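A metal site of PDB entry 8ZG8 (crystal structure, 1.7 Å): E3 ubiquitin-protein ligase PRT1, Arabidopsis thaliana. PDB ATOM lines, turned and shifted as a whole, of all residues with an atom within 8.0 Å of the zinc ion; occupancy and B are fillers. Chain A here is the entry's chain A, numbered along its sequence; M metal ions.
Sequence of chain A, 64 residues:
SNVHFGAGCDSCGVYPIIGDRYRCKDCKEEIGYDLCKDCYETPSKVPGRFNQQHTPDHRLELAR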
ATOM      1  N   ARG A  23       7.610 -19.241  27.263  1.00  0.00           N
ATOM      2  CA  ARG A  23       7.626 -19.284  25.823  1.00  0.00           C
ATOM      3  C   ARG A  23       6.536 -18.374  25.256  1.00  0.00           C
ATOM      4  O   ARG A  23       5.399 -18.419  25.741  1.00  0.00           O
ATOM      5  CB  ARG A  23       7.297 -20.716  25.345  1.00  0.00           C
ATOM      6  CG  ARG A  23       7.364 -20.797  23.846  1.00  0.00           C
ATOM      7  CD  ARG A  23       7.052 -22.201  23.493  1.00  0.00           C
ATOM      8  NE  ARG A  23       8.064 -23.114  23.125  1.00  0.00           N
ATOM      9  CZ  ARG A  23       8.156 -23.644  21.927  1.00  0.00           C
ATOM     10  NH1 ARG A  23       7.271 -23.347  20.981  1.00  0.00           N
ATOM     11  NH2 ARG A  23       9.153 -24.482  21.691  1.00  0.00           N
ATOM     12  N   CYS A  24       6.864 -17.500  24.289  1.00  0.00           N
ATOM     13  CA  CYS A  24       5.852 -16.572  23.768  1.00  0.00           C
ATOM     14  C   CYS A  24       4.789 -17.308  22.959  1.00  0.00           C
ATOM     15  O   CYS A  24       5.110 -18.094  22.057  1.00  0.00           O
ATOM     16  CB  CYS A  24       6.488 -15.495  22.889  1.00  0.00           C
ATOM     17  SG  CYS A  24       5.208 -14.298  22.420  1.00  0.00           S
ATOM     18  N   LYS A  25       3.520 -17.020  23.253  1.00  0.00           N
ATOM     19  CA  LYS A  25       2.421 -17.660  22.532  1.00  0.00           C
ATOM     20  C   LYS A  25       2.161 -16.991  21.188  1.00  0.00           C
ATOM     21  O   LYS A  25       1.755 -17.655  20.230  1.00  0.00           O
ATOM     22  CB  LYS A  25       1.159 -17.620  23.394  1.00  0.00           C
ATOM     23  CG  LYS A  25       1.179 -18.546  24.596  1.00  0.00           C
ATOM     24  CD  LYS A  25       0.687 -19.957  24.257  1.00  0.00           C
ATOM     25  CE  LYS A  25       0.980 -20.932  25.396  1.00  0.00           C
ATOM     26  NZ  LYS A  25      -0.166 -21.780  25.805  1.00  0.00           N
ATOM     27  N   ASP A  26       2.378 -15.669  21.111  1.00  0.00           N
ATOM     28  CA  ASP A  26       2.110 -14.889  19.899  1.00  0.00           C
ATOM     29  C   ASP A  26       3.170 -15.152  18.833  1.00  0.00           C
ATOM     30  O   ASP A  26       2.842 -15.513  17.696  1.00  0.00           O
ATOM     31  CB  ASP A  26       1.968 -13.426  20.315  1.00  0.00           C
ATOM     32  CG  ASP A  26       0.921 -13.261  21.441  1.00  0.00           C
ATOM     33  OD1 ASP A  26      -0.157 -13.852  21.301  1.00  0.00           O
ATOM     34  OD2 ASP A  26       1.166 -12.610  22.466  1.00  0.00           O
ATOM     35  N   CYS A  27       4.451 -14.918  19.158  1.00  0.00           N
ATOM     36  CA  CYS A  27       5.550 -15.361  18.295  1.00  0.00           C
ATOM     37  C   CYS A  27       5.359 -16.866  18.021  1.00  0.00           C
ATOM     38  O   CYS A  27       6.028 -17.448  17.172  1.00  0.00           O
ATOM     39  CB  CYS A  27       6.919 -15.074  18.910  1.00  0.00           C
ATOM     40  SG  CYS A  27       7.300 -13.267  19.093  1.00  0.00           S
ATOM     41  N   GLY A  32       9.878 -17.513  17.256  1.00  0.00           N
ATOM     42  CA  GLY A  32       9.844 -17.990  18.618  1.00  0.00           C
ATOM     43  C   GLY A  32      10.573 -16.996  19.506  1.00  0.00           C
ATOM     44  O   GLY A  32      11.490 -16.291  19.077  1.00  0.00           O
ATOM     45  N   TYR A  33      10.161 -16.945  20.755  1.00  0.00           N
ATOM     46  CA  TYR A  33      10.747 -16.017  21.706  1.00  0.00           C
ATOM     47  C   TYR A  33      10.597 -16.664  23.062  1.00  0.00           C
ATOM     48  O   TYR A  33       9.498 -17.061  23.428  1.00  0.00           O
ATOM     49  CB  TYR A  33      10.054 -14.669  21.622  1.00  0.00           C
ATOM     50  CG  TYR A  33      10.645 -13.614  22.523  1.00  0.00           C
ATOM     51  CD1 TYR A  33      10.258 -13.501  23.860  1.00  0.00           C
ATOM     52  CD2 TYR A  33      11.616 -12.746  22.041  1.00  0.00           C
ATOM     53  CE1 TYR A  33      10.806 -12.536  24.702  1.00  0.00           C
ATOM     54  CE2 TYR A  33      12.191 -11.762  22.850  1.00  0.00           C
ATOM     55  CZ  TYR A  33      11.767 -11.650  24.183  1.00  0.00           C
ATOM     56  OH  TYR A  33      12.320 -10.691  25.004  1.00  0.00           O
ATOM     57  N   ASP A  34      11.679 -16.742  23.803  1.00  0.00           N
ATOM     58  CA  ASP A  34      11.711 -17.435  25.089  1.00  0.00           C
ATOM     59  C   ASP A  34      12.367 -16.544  26.124  1.00  0.00           C
ATOM     60  O   ASP A  34      13.253 -15.765  25.776  1.00  0.00           O
ATOM     61  CB  ASP A  34      12.584 -18.705  25.049  1.00  0.00           C
ATOM     62  CG  ASP A  34      12.136 -19.660  24.056  1.00  0.00           C
ATOM     63  OD1 ASP A  34      11.118 -20.340  24.302  1.00  0.00           O
ATOM     64  OD2 ASP A  34      12.821 -19.799  23.041  1.00  0.00           O
ATOM     65  N   ARG A  49      12.640  -6.229  24.065  1.00  0.00           N
ATOM     66  CA  ARG A  49      11.627  -6.109  23.042  1.00  0.00           C
ATOM     67  C   ARG A  49      12.258  -5.602  21.744  1.00  0.00           C
ATOM     68  O   ARG A  49      13.284  -4.928  21.758  1.00  0.00           O
ATOM     69  CB  ARG A  49      10.491  -5.160  23.462  1.00  0.00           C
ATOM     70  CG  ARG A  49      10.135  -5.138  24.923  1.00  0.00           C
ATOM     71  CD  ARG A  49       9.192  -6.248  25.290  1.00  0.00           C
ATOM     72  NE  ARG A  49       8.960  -6.206  26.730  1.00  0.00           N
ATOM     73  CZ  ARG A  49       7.998  -6.865  27.359  1.00  0.00           C
ATOM     74  NH1 ARG A  49       7.857  -6.751  28.670  1.00  0.00           N
ATOM     75  NH2 ARG A  49       7.189  -7.665  26.678  1.00  0.00           N
ATOM     76  N   GLN A  53       9.854  -8.970  16.281  1.00  0.00           N
ATOM     77  CA  GLN A  53       8.499  -9.490  16.211  1.00  0.00           C
ATOM     78  C   GLN A  53       7.775  -9.516  17.545  1.00  0.00           C
ATOM     79  O   GLN A  53       6.551  -9.472  17.548  1.00  0.00           O
ATOM     80  CB  GLN A  53       8.567 -10.919  15.645  1.00  0.00           C
ATOM     81  CG  GLN A  53       9.170 -10.963  14.252  1.00  0.00           C
ATOM     82  CD  GLN A  53       9.224 -12.349  13.633  1.00  0.00           C
ATOM     83  OE1 GLN A  53       9.272 -13.367  14.334  1.00  0.00           O
ATOM     84  NE2 GLN A  53       9.162 -12.397  12.309  1.00  0.00           N
ATOM     85  N   HIS A  54       8.492  -9.408  18.656  1.00  0.00           N
ATOM     86  CA  HIS A  54       7.946  -9.551  20.002  1.00  0.00           C
ATOM     87  C   HIS A  54       7.740  -8.192  20.647  1.00  0.00           C
ATOM     88  O   HIS A  54       8.692  -7.473  20.941  1.00  0.00           O
ATOM     89  CB  HIS A  54       8.895 -10.436  20.825  1.00  0.00           C
ATOM     90  CG  HIS A  54       8.370 -10.760  22.171  1.00  0.00           C
ATOM     91  ND1 HIS A  54       7.387 -11.693  22.359  1.00  0.00           N
ATOM     92  CD2 HIS A  54       8.673 -10.257  23.385  1.00  0.00           C
ATOM     93  CE1 HIS A  54       7.165 -11.807  23.660  1.00  0.00           C
ATOM     94  NE2 HIS A  54       7.876 -10.888  24.290  1.00  0.00           N
ATOM     95  N   THR A  55       6.468  -7.836  20.854  1.00  0.00           N
ATOM     96  CA  THR A  55       6.061  -6.580  21.445  1.00  0.00           C
ATOM     97  C   THR A  55       5.657  -6.796  22.897  1.00  0.00           C
ATOM     98  O   THR A  55       5.459  -7.924  23.346  1.00  0.00           O
ATOM     99  CB  THR A  55       4.924  -5.943  20.646  1.00  0.00           C
ATOM    100  OG1 THR A  55       3.909  -6.897  20.305  1.00  0.00           O
ATOM    101  CG2 THR A  55       5.509  -5.377  19.369  1.00  0.00           C
ATOM    102  N   PRO A  56       5.533  -5.711  23.662  1.00  0.00           N
ATOM    103  CA  PRO A  56       5.038  -5.879  25.051  1.00  0.00           C
ATOM    104  C   PRO A  56       3.599  -6.398  25.118  1.00  0.00           C
ATOM    105  O   PRO A  56       3.224  -6.985  26.154  1.00  0.00           O
ATOM    106  CB  PRO A  56       5.119  -4.448  25.616  1.00  0.00           C
ATOM    107  CG  PRO A  56       6.155  -3.729  24.720  1.00  0.00           C
ATOM    108  CD  PRO A  56       5.934  -4.328  23.352  1.00  0.00           C
ATOM    109  N   ASP A  57       2.856  -6.337  24.006  1.00  0.00           N
ATOM    110  CA  ASP A  57       1.508  -6.906  23.947  1.00  0.00           C
ATOM    111  C   ASP A  57       1.517  -8.435  24.020  1.00  0.00           C
ATOM    112  O   ASP A  57       0.470  -9.039  24.286  1.00  0.00           O
ATOM    113  CB  ASP A  57       0.843  -6.513  22.614  1.00  0.00           C
ATOM    114  CG  ASP A  57       0.479  -5.031  22.527  1.00  0.00           C
ATOM    115  OD1 ASP A  57       0.052  -4.429  23.534  1.00  0.00           O
ATOM    116  OD2 ASP A  57       0.630  -4.460  21.422  1.00  0.00           O
ATOM    117  N   HIS A  58       2.676  -9.060  23.807  1.00  0.00           N
ATOM    118  CA  HIS A  58       2.787 -10.496  23.682  1.00  0.00           C
ATOM    119  C   HIS A  58       2.701 -11.117  25.058  1.00  0.00           C
ATOM    120  O   HIS A  58       3.168 -10.554  26.049  1.00  0.00           O
ATOM    121  CB  HIS A  58       4.127 -10.847  22.993  1.00  0.00           C
ATOM    122  CG  HIS A  58       4.075 -10.676  21.500  1.00  0.00           C
ATOM    123  ND1 HIS A  58       4.794 -11.478  20.640  1.00  0.00           N
ATOM    124  CD2 HIS A  58       3.370  -9.823  20.717  1.00  0.00           C
ATOM    125  CE1 HIS A  58       4.567 -11.117  19.396  1.00  0.00           C
ATOM    126  NE2 HIS A  58       3.696 -10.123  19.405  1.00  0.00           N
ATOM    127  N   ARG A  59       2.082 -12.293  25.113  1.00  0.00           N
ATOM    128  CA  ARG A  59       1.983 -13.068  26.345  1.00  0.00           C
ATOM    129  C   ARG A  59       2.811 -14.347  26.260  1.00  0.00           C
ATOM    130  O   ARG A  59       2.727 -15.106  25.283  1.00  0.00           O
ATOM    131  CB  ARG A  59       0.528 -13.421  26.647  1.00  0.00           C
ATOM    132  CG  ARG A  59      -0.046 -14.401  25.662  1.00  0.00           C
ATOM    133  CD  ARG A  59      -1.492 -14.707  25.991  1.00  0.00           C
ATOM    134  NE  ARG A  59      -1.601 -15.856  26.866  1.00  0.00           N
ATOM    135  CZ  ARG A  59      -1.819 -17.092  26.438  1.00  0.00           C
ATOM    136  NH1 ARG A  59      -1.954 -17.339  25.146  1.00  0.00           N
ATOM    137  NH2 ARG A  59      -1.922 -18.084  27.312  1.00  0.00           N
ATOM    138  N   LEU A  60       3.508 -14.644  27.339  1.00  0.00           N
ATOM    139  CA  LEU A  60       4.305 -15.855  27.436  1.00  0.00           C
ATOM    140  C   LEU A  60       3.743 -16.771  28.519  1.00  0.00           C
ATOM    141  O   LEU A  60       3.144 -16.309  29.499  1.00  0.00           O
ATOM    142  CB  LEU A  60       5.720 -15.531  27.804  1.00  0.00           C
ATOM    143  CG  LEU A  60       6.444 -14.520  26.912  1.00  0.00           C
ATOM    144  CD1 LEU A  60       6.246 -13.100  27.441  1.00  0.00           C
ATOM    145  CD2 LEU A  60       7.912 -14.860  26.891  1.00  0.00           C
HETATM  146 ZN    ZN M   1       6.304 -12.734  21.115  1.00  0.00          ZN
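Of the 17 residues printed, 4 come within 4 Å of the zinc ion. The nearest printed residue that does not touch the zinc ion is Tyr 33 (4.3 Å).
The zinc ion is bound by a ring nitrogen (ND1) of His 54 (2.0 Å), a ring nitrogen (ND1) of His 58 (2.0 Å), the side-chain sulfur of Cys 24 (2.3 Å) and the side-chain sulfur of Cys 27 (2.3 Å). The zinc ion has four donor atoms within binding distance.
A ring nitrogen (NE2) of His 58 lies close to the backbone carbonyl oxygen (O) of Gln 53 (3.5 Å). OG1 of Thr 55 sits close to NE2 of His 58 (3.4 Å). O of Tyr 33 lies within hydrogen-bond range of N of Cys 24. N of Asp 26 lies close to SG of Cys 24, at 3.4 Å.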
